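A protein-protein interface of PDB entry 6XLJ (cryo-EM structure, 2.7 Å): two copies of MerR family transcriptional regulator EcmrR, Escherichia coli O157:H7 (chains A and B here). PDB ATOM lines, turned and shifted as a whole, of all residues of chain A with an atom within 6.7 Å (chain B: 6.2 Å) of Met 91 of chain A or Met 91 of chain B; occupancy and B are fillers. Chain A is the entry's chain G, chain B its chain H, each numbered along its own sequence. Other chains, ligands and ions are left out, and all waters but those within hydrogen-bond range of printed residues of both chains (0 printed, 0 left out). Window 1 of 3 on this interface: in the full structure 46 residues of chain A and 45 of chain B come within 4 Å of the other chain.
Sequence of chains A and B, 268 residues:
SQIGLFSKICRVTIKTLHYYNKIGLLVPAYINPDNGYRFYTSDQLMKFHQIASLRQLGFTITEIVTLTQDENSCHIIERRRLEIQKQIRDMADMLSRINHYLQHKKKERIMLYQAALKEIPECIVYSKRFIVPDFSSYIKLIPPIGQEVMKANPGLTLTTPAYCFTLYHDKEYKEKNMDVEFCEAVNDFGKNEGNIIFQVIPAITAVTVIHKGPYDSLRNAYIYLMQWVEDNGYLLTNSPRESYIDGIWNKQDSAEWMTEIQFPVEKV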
ATOM      1  N   ILE A  84      25.730 -29.849  -4.924  1.00  0.00           N
ATOM      2  CA  ILE A  84      24.817 -29.645  -3.803  1.00  0.00           C
ATOM      3  C   ILE A  84      24.964 -28.224  -3.283  1.00  0.00           C
ATOM      4  O   ILE A  84      23.984 -27.608  -2.851  1.00  0.00           O
ATOM      5  CB  ILE A  84      24.955 -30.724  -2.708  1.00  0.00           C
ATOM      6  CG1 ILE A  84      23.808 -30.594  -1.700  1.00  0.00           C
ATOM      7  CG2 ILE A  84      26.227 -30.636  -1.951  1.00  0.00           C
ATOM      8  CD1 ILE A  84      22.437 -30.806  -2.288  1.00  0.00           C
ATOM      9  N   LYS A  86      25.652 -25.677  -5.145  1.00  0.00           N
ATOM     10  CA  LYS A  86      24.880 -24.870  -6.081  1.00  0.00           C
ATOM     11  C   LYS A  86      23.376 -24.985  -5.824  1.00  0.00           C
ATOM     12  O   LYS A  86      22.666 -23.974  -5.850  1.00  0.00           O
ATOM     13  CB  LYS A  86      25.260 -25.203  -7.529  1.00  0.00           C
ATOM     14  CG  LYS A  86      24.658 -24.366  -8.624  1.00  0.00           C
ATOM     15  CD  LYS A  86      24.733 -25.100  -9.929  1.00  0.00           C
ATOM     16  CE  LYS A  86      26.152 -25.517 -10.184  1.00  0.00           C
ATOM     17  NZ  LYS A  86      26.261 -26.116 -11.538  1.00  0.00           N
ATOM     18  N   GLN A  87      22.865 -26.198  -5.564  1.00  0.00           N
ATOM     19  CA  GLN A  87      21.428 -26.300  -5.311  1.00  0.00           C
ATOM     20  C   GLN A  87      21.019 -25.678  -3.987  1.00  0.00           C
ATOM     21  O   GLN A  87      19.887 -25.211  -3.867  1.00  0.00           O
ATOM     22  CB  GLN A  87      20.913 -27.743  -5.344  1.00  0.00           C
ATOM     23  CG  GLN A  87      20.809 -28.330  -6.732  1.00  0.00           C
ATOM     24  CD  GLN A  87      21.768 -29.471  -6.944  1.00  0.00           C
ATOM     25  OE1 GLN A  87      22.485 -29.864  -6.034  1.00  0.00           O
ATOM     26  NE2 GLN A  87      21.831 -29.973  -8.169  1.00  0.00           N
ATOM     27  N   ILE A  88      21.903 -25.650  -2.990  1.00  0.00           N
ATOM     28  CA  ILE A  88      21.562 -24.942  -1.759  1.00  0.00           C
ATOM     29  C   ILE A  88      21.469 -23.442  -2.028  1.00  0.00           C
ATOM     30  O   ILE A  88      20.550 -22.774  -1.535  1.00  0.00           O
ATOM     31  CB  ILE A  88      22.486 -25.317  -0.575  1.00  0.00           C
ATOM     32  CG1 ILE A  88      21.837 -24.876   0.736  1.00  0.00           C
ATOM     33  CG2 ILE A  88      23.854 -24.700  -0.624  1.00  0.00           C
ATOM     34  CD1 ILE A  88      20.399 -25.318   0.893  1.00  0.00           C
ATOM     35  N   ARG A  89      22.426 -22.884  -2.784  1.00  0.00           N
ATOM     36  CA  ARG A  89      22.330 -21.469  -3.149  1.00  0.00           C
ATOM     37  C   ARG A  89      21.040 -21.194  -3.910  1.00  0.00           C
ATOM     38  O   ARG A  89      20.321 -20.224  -3.618  1.00  0.00           O
ATOM     39  CB  ARG A  89      23.529 -21.045  -3.993  1.00  0.00           C
ATOM     40  CG  ARG A  89      24.877 -21.187  -3.318  1.00  0.00           C
ATOM     41  CD  ARG A  89      25.986 -20.927  -4.315  1.00  0.00           C
ATOM     42  NE  ARG A  89      27.301 -21.316  -3.821  1.00  0.00           N
ATOM     43  CZ  ARG A  89      28.034 -22.286  -4.349  1.00  0.00           C
ATOM     44  NH1 ARG A  89      29.223 -22.576  -3.841  1.00  0.00           N
ATOM     45  NH2 ARG A  89      27.579 -22.966  -5.391  1.00  0.00           N
ATOM     46  N   ASP A  90      20.719 -22.059  -4.872  1.00  0.00           N
ATOM     47  CA  ASP A  90      19.536 -21.860  -5.695  1.00  0.00           C
ATOM     48  C   ASP A  90      18.271 -21.997  -4.861  1.00  0.00           C
ATOM     49  O   ASP A  90      17.309 -21.252  -5.053  1.00  0.00           O
ATOM     50  CB  ASP A  90      19.545 -22.853  -6.861  1.00  0.00           C
ATOM     51  CG  ASP A  90      18.410 -22.625  -7.850  1.00  0.00           C
ATOM     52  OD1 ASP A  90      18.702 -22.250  -9.004  1.00  0.00           O
ATOM     53  OD2 ASP A  90      17.237 -22.860  -7.498  1.00  0.00           O
ATOM     54  N   MET A  91      18.251 -22.933  -3.923  1.00  0.00           N
ATOM     55  CA  MET A  91      17.061 -23.100  -3.109  1.00  0.00           C
ATOM     56  C   MET A  91      16.887 -21.945  -2.134  1.00  0.00           C
ATOM     57  O   MET A  91      15.754 -21.566  -1.839  1.00  0.00           O
ATOM     58  CB  MET A  91      17.085 -24.431  -2.382  1.00  0.00           C
ATOM     59  CG  MET A  91      15.695 -24.842  -1.966  1.00  0.00           C
ATOM     60  SD  MET A  91      14.635 -25.126  -3.389  1.00  0.00           S
ATOM     61  CE  MET A  91      15.330 -26.654  -4.017  1.00  0.00           C
ATOM     62  N   ALA A  92      17.979 -21.397  -1.589  1.00  0.00           N
ATOM     63  CA  ALA A  92      17.841 -20.219  -0.735  1.00  0.00           C
ATOM     64  C   ALA A  92      17.314 -19.023  -1.523  1.00  0.00           C
ATOM     65  O   ALA A  92      16.483 -18.253  -1.016  1.00  0.00           O
ATOM     66  CB  ALA A  92      19.181 -19.878  -0.088  1.00  0.00           C
ATOM     67  N   ASP A  93      17.772 -18.858  -2.771  1.00  0.00           N
ATOM     68  CA  ASP A  93      17.209 -17.789  -3.595  1.00  0.00           C
ATOM     69  C   ASP A  93      15.723 -18.056  -3.815  1.00  0.00           C
ATOM     70  O   ASP A  93      14.912 -17.129  -3.765  1.00  0.00           O
ATOM     71  CB  ASP A  93      18.009 -17.503  -4.886  1.00  0.00           C
ATOM     72  CG  ASP A  93      17.861 -18.533  -5.982  1.00  0.00           C
ATOM     73  OD1 ASP A  93      16.736 -18.920  -6.362  1.00  0.00           O
ATOM     74  OD2 ASP A  93      18.914 -18.897  -6.537  1.00  0.00           O
ATOM     75  N   MET A  94      15.365 -19.314  -4.111  1.00  0.00           N
ATOM     76  CA  MET A  94      13.961 -19.692  -4.268  1.00  0.00           C
ATOM     77  C   MET A  94      13.171 -19.359  -3.008  1.00  0.00           C
ATOM     78  O   MET A  94      12.002 -18.971  -3.087  1.00  0.00           O
ATOM     79  CB  MET A  94      13.849 -21.191  -4.529  1.00  0.00           C
ATOM     80  CG  MET A  94      14.266 -21.675  -5.890  1.00  0.00           C
ATOM     81  SD  MET A  94      13.198 -21.207  -7.246  1.00  0.00           S
ATOM     82  CE  MET A  94      13.844 -22.296  -8.508  1.00  0.00           C
ATOM     83  N   LEU A  95      13.781 -19.546  -1.838  1.00  0.00           N
ATOM     84  CA  LEU A  95      13.109 -19.209  -0.588  1.00  0.00           C
ATOM     85  C   LEU A  95      12.818 -17.723  -0.533  1.00  0.00           C
ATOM     86  O   LEU A  95      11.719 -17.308  -0.150  1.00  0.00           O
ATOM     87  CB  LEU A  95      13.957 -19.628   0.617  1.00  0.00           C
ATOM     88  CG  LEU A  95      13.393 -19.251   1.996  1.00  0.00           C
ATOM     89  CD1 LEU A  95      13.542 -20.328   3.029  1.00  0.00           C
ATOM     90  CD2 LEU A  95      14.153 -18.025   2.513  1.00  0.00           C
ATOM     91  N   SER A  96      13.807 -16.905  -0.886  1.00  0.00           N
ATOM     92  CA  SER A  96      13.576 -15.464  -0.891  1.00  0.00           C
ATOM     93  C   SER A  96      12.499 -15.086  -1.903  1.00  0.00           C
ATOM     94  O   SER A  96      11.633 -14.249  -1.620  1.00  0.00           O
ATOM     95  CB  SER A  96      14.878 -14.737  -1.209  1.00  0.00           C
ATOM     96  OG  SER A  96      15.407 -15.196  -2.442  1.00  0.00           O
ATOM     97  N   ARG B  80       3.837 -24.749  -0.922  1.00  0.00           N
ATOM     98  CA  ARG B  80       5.113 -24.857  -1.633  1.00  0.00           C
ATOM     99  C   ARG B  80       6.251 -24.257  -0.825  1.00  0.00           C
ATOM    100  O   ARG B  80       7.389 -24.737  -0.895  1.00  0.00           O
ATOM    101  CB  ARG B  80       5.015 -24.193  -3.003  1.00  0.00           C
ATOM    102  CG  ARG B  80       6.322 -24.142  -3.788  1.00  0.00           C
ATOM    103  CD  ARG B  80       6.831 -25.498  -4.221  1.00  0.00           C
ATOM    104  NE  ARG B  80       8.260 -25.423  -4.501  1.00  0.00           N
ATOM    105  CZ  ARG B  80       9.039 -26.467  -4.755  1.00  0.00           C
ATOM    106  NH1 ARG B  80      10.331 -26.293  -4.992  1.00  0.00           N
ATOM    107  NH2 ARG B  80       8.527 -27.688  -4.772  1.00  0.00           N
ATOM    108  N   ILE B  84       9.646 -26.220   0.238  1.00  0.00           N
ATOM    109  CA  ILE B  84      10.992 -25.728  -0.018  1.00  0.00           C
ATOM    110  C   ILE B  84      11.786 -25.644   1.278  1.00  0.00           C
ATOM    111  O   ILE B  84      12.976 -25.963   1.298  1.00  0.00           O
ATOM    112  CB  ILE B  84      10.920 -24.364  -0.725  1.00  0.00           C
ATOM    113  CG1 ILE B  84      10.358 -24.530  -2.128  1.00  0.00           C
ATOM    114  CG2 ILE B  84      12.295 -23.760  -0.853  1.00  0.00           C
ATOM    115  CD1 ILE B  84      10.231 -23.240  -2.887  1.00  0.00           C
ATOM    116  N   LYS B  86      11.402 -27.680   3.875  1.00  0.00           N
ATOM    117  CA  LYS B  86      11.805 -29.060   4.139  1.00  0.00           C
ATOM    118  C   LYS B  86      13.012 -29.443   3.294  1.00  0.00           C
ATOM    119  O   LYS B  86      13.954 -30.081   3.787  1.00  0.00           O
ATOM    120  CB  LYS B  86      10.646 -30.000   3.789  1.00  0.00           C
ATOM    121  CG  LYS B  86       9.359 -29.881   4.589  1.00  0.00           C
ATOM    122  CD  LYS B  86       9.371 -30.675   5.867  1.00  0.00           C
ATOM    123  CE  LYS B  86       9.205 -32.155   5.597  1.00  0.00           C
ATOM    124  NZ  LYS B  86       9.436 -32.966   6.824  1.00  0.00           N
ATOM    125  N   GLN B  87      13.020 -29.027   2.027  1.00  0.00           N
ATOM    126  CA  GLN B  87      14.137 -29.389   1.163  1.00  0.00           C
ATOM    127  C   GLN B  87      15.418 -28.686   1.581  1.00  0.00           C
ATOM    128  O   GLN B  87      16.486 -29.294   1.548  1.00  0.00           O
ATOM    129  CB  GLN B  87      13.839 -29.165  -0.321  1.00  0.00           C
ATOM    130  CG  GLN B  87      12.827 -30.163  -0.883  1.00  0.00           C
ATOM    131  CD  GLN B  87      11.573 -29.549  -1.439  1.00  0.00           C
ATOM    132  OE1 GLN B  87      11.530 -28.361  -1.739  1.00  0.00           O
ATOM    133  NE2 GLN B  87      10.524 -30.353  -1.555  1.00  0.00           N
ATOM    134  N   ILE B  88      15.335 -27.417   1.990  1.00  0.00           N
ATOM    135  CA  ILE B  88      16.535 -26.715   2.447  1.00  0.00           C
ATOM    136  C   ILE B  88      17.101 -27.364   3.692  1.00  0.00           C
ATOM    137  O   ILE B  88      18.321 -27.534   3.815  1.00  0.00           O
ATOM    138  CB  ILE B  88      16.240 -25.230   2.729  1.00  0.00           C
ATOM    139  CG1 ILE B  88      15.684 -24.523   1.509  1.00  0.00           C
ATOM    140  CG2 ILE B  88      17.496 -24.511   3.199  1.00  0.00           C
ATOM    141  CD1 ILE B  88      14.745 -23.427   1.851  1.00  0.00           C
ATOM    142  N   ARG B  89      16.233 -27.765   4.618  1.00  0.00           N
ATOM    143  CA  ARG B  89      16.724 -28.428   5.820  1.00  0.00           C
ATOM    144  C   ARG B  89      17.415 -29.742   5.474  1.00  0.00           C
ATOM    145  O   ARG B  89      18.533 -30.018   5.941  1.00  0.00           O
ATOM    146  CB  ARG B  89      15.571 -28.650   6.791  1.00  0.00           C
ATOM    147  CG  ARG B  89      15.946 -29.447   8.014  1.00  0.00           C
ATOM    148  CD  ARG B  89      14.852 -29.408   9.066  1.00  0.00           C
ATOM    149  NE  ARG B  89      13.555 -29.818   8.544  1.00  0.00           N
ATOM    150  CZ  ARG B  89      12.532 -28.992   8.373  1.00  0.00           C
ATOM    151  NH1 ARG B  89      12.645 -27.709   8.677  1.00  0.00           N
ATOM    152  NH2 ARG B  89      11.393 -29.452   7.904  1.00  0.00           N
ATOM    153  N   ASP B  90      16.796 -30.530   4.593  1.00  0.00           N
ATOM    154  CA  ASP B  90      17.375 -31.813   4.225  1.00  0.00           C
ATOM    155  C   ASP B  90      18.646 -31.651   3.400  1.00  0.00           C
ATOM    156  O   ASP B  90      19.571 -32.461   3.524  1.00  0.00           O
ATOM    157  CB  ASP B  90      16.333 -32.616   3.457  1.00  0.00           C
ATOM    158  CG  ASP B  90      15.168 -33.033   4.333  1.00  0.00           C
ATOM    159  OD1 ASP B  90      15.374 -33.212   5.550  1.00  0.00           O
ATOM    160  OD2 ASP B  90      14.039 -33.150   3.809  1.00  0.00           O
ATOM    161  N   MET B  91      18.722 -30.611   2.574  1.00  0.00           N
ATOM    162  CA  MET B  91      19.926 -30.353   1.791  1.00  0.00           C
ATOM    163  C   MET B  91      21.073 -29.875   2.667  1.00  0.00           C
ATOM    164  O   MET B  91      22.232 -30.203   2.408  1.00  0.00           O
ATOM    165  CB  MET B  91      19.633 -29.365   0.669  1.00  0.00           C
ATOM    166  CG  MET B  91      18.857 -29.997  -0.467  1.00  0.00           C
ATOM    167  SD  MET B  91      18.604 -28.870  -1.833  1.00  0.00           S
ATOM    168  CE  MET B  91      17.361 -27.825  -1.119  1.00  0.00           C
ATOM    169  N   ALA B  92      20.779 -29.066   3.687  1.00  0.00           N
ATOM    170  CA  ALA B  92      21.831 -28.678   4.622  1.00  0.00           C
ATOM    171  C   ALA B  92      22.354 -29.894   5.375  1.00  0.00           C
ATOM    172  O   ALA B  92      23.569 -30.035   5.588  1.00  0.00           O
ATOM    173  CB  ALA B  92      21.305 -27.621   5.590  1.00  0.00           C
ATOM    174  N   ASP B  93      21.443 -30.789   5.770  1.00  0.00           N
ATOM    175  CA  ASP B  93      21.850 -32.063   6.358  1.00  0.00           C
ATOM    176  C   ASP B  93      22.777 -32.814   5.411  1.00  0.00           C
ATOM    177  O   ASP B  93      23.873 -33.237   5.797  1.00  0.00           O
ATOM    178  CB  ASP B  93      20.619 -32.906   6.687  1.00  0.00           C
ATOM    179  CG  ASP B  93      20.956 -34.174   7.462  1.00  0.00           C
ATOM    180  OD1 ASP B  93      20.015 -34.937   7.765  1.00  0.00           O
ATOM    181  OD2 ASP B  93      22.138 -34.415   7.785  1.00  0.00           O
ATOM    182  N   MET B  94      22.334 -32.989   4.165  1.00  0.00           N
ATOM    183  CA  MET B  94      23.104 -33.706   3.156  1.00  0.00           C
ATOM    184  C   MET B  94      24.471 -33.062   2.944  1.00  0.00           C
ATOM    185  O   MET B  94      25.463 -33.760   2.709  1.00  0.00           O
ATOM    186  CB  MET B  94      22.281 -33.764   1.873  1.00  0.00           C
ATOM    187  CG  MET B  94      22.827 -34.633   0.782  1.00  0.00           C
ATOM    188  SD  MET B  94      21.973 -34.281  -0.763  1.00  0.00           S
ATOM    189  CE  MET B  94      20.373 -35.013  -0.420  1.00  0.00           C
ATOM    190  N   LEU B  95      24.533 -31.734   2.987  1.00  0.00           N
ATOM    191  CA  LEU B  95      25.798 -31.038   2.791  1.00  0.00           C
ATOM    192  C   LEU B  95      26.753 -31.324   3.941  1.00  0.00           C
ATOM    193  O   LEU B  95      27.958 -31.524   3.731  1.00  0.00           O
ATOM    194  CB  LEU B  95      25.556 -29.540   2.652  1.00  0.00           C
ATOM    195  CG  LEU B  95      26.779 -28.665   2.389  1.00  0.00           C
ATOM    196  CD1 LEU B  95      27.492 -29.024   1.090  1.00  0.00           C
ATOM    197  CD2 LEU B  95      26.310 -27.222   2.381  1.00  0.00           C
ATOM    198  N   SER B  96      26.234 -31.324   5.168  1.00  0.00           N
ATOM    199  CA  SER B  96      27.083 -31.671   6.299  1.00  0.00           C
ATOM    200  C   SER B  96      27.585 -33.102   6.166  1.00  0.00           C
ATOM    201  O   SER B  96      28.762 -33.385   6.433  1.00  0.00           O
ATOM    202  CB  SER B  96      26.317 -31.492   7.607  1.00  0.00           C
ATOM    203  OG  SER B  96      25.255 -32.425   7.704  1.00  0.00           O
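The side-chain amide oxygen (OE1) of Gln 87 of chain A lies close to the backbone NH (N) of Ile 84 of chain A (3.4 Å).
The backbone NH (N) of Ile 84 of chain B sits close to the side-chain amide oxygen (OE1) of Gln 87 of chain B (3.5 Å).
Of the 13 printed residues of chain B, 5 touch a printed residue of chain A.
Printed residues of chain B that touch a printed residue of chain A: Ile 84, Ile 88, Met 91, Met 94 and Leu 95.
Hydrophobic or aromatic side chains of chain B within 4 Å of the printed part of chain A: Ile 84, Ile 88, Met 91, Met 94 and Leu 95.
Hydrophobic or aromatic side chains of chain A within 4 Å of the printed part of chain B: Ile 84, Ile 88, Met 91 and Leu 95.
Among the printed residues, 7 pairs touch across the chains.
Among the printed residues, no Asp or Glu carboxylate lies within 4 Å of a Lys or Arg side-chain nitrogen of the other chain.
Ile 84 of chain A touches Leu 95 of chain B, but with the chains exchanged Leu 95 of chain A does not touch Ile 84 of chain B (4.6 Å).
Met 91 of chain A touches Ile 84 of chain B, but with the chains exchanged Ile 84 of chain A does not touch Met 91 of chain B (4.1 Å).
Met 91 of chain A touches Ile 88 of chain B, but with the chains exchanged Ile 88 of chain A does not touch Met 91 of chain B (4.1 Å).
Met 91 of chain A touches its own counterpart, Met 91 of chain B.
Positions printed for both chains: 84, 86, 87, 88, 89, 90, 91, 92, 93, 94, 95 and 96.
Of the 7 pairs that touch across the chains among the printed residues, 2 have their exchanged pair printed and touching as well.
Met 91 of chain A touches three residues of chain B.
Met 91 of chain B touches one residue of chain A.
Printed residues of chain A within 4 Å of Met 94 of chain B: Ile 84 (3.8 Å).
Of the printed residues of chain B, Leu 95 of chain A touches Ile 88 (3.5 Å).
Of the printed residues of chain B, Ile 88 of chain A touches Ile 88.
Gln 87 of chain B touches none of the printed residues of chain A.
The nearest printed residue of chain B that does not touch Met 91 of chain A is Gln 87 of chain B (4.7 Å).
The nearest printed residue of chain A that does not touch Met 94 of chain B is Gln 87 of chain A (6.9 Å).
Ile 84 of chain A touches Met 94 of chain B (CD1 to SD, 3.8 Å).
Ile 84 of chain A touches Leu 95 of chain B.
Ile 88 of chain B touches Ile 88 of chain A (CG2 to CD1, 3.8 Å).
Ile 84 of chain B touches Met 91 of chain A (CG2 to SD, 3.7 Å).
CG of Met 91 of chain A touches CG1 of Ile 88 of chain B (3.5 Å).
Met 91 of chain B touches Met 91 of chain A.
Leu 95 of chain A touches Ile 88 of chain B.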
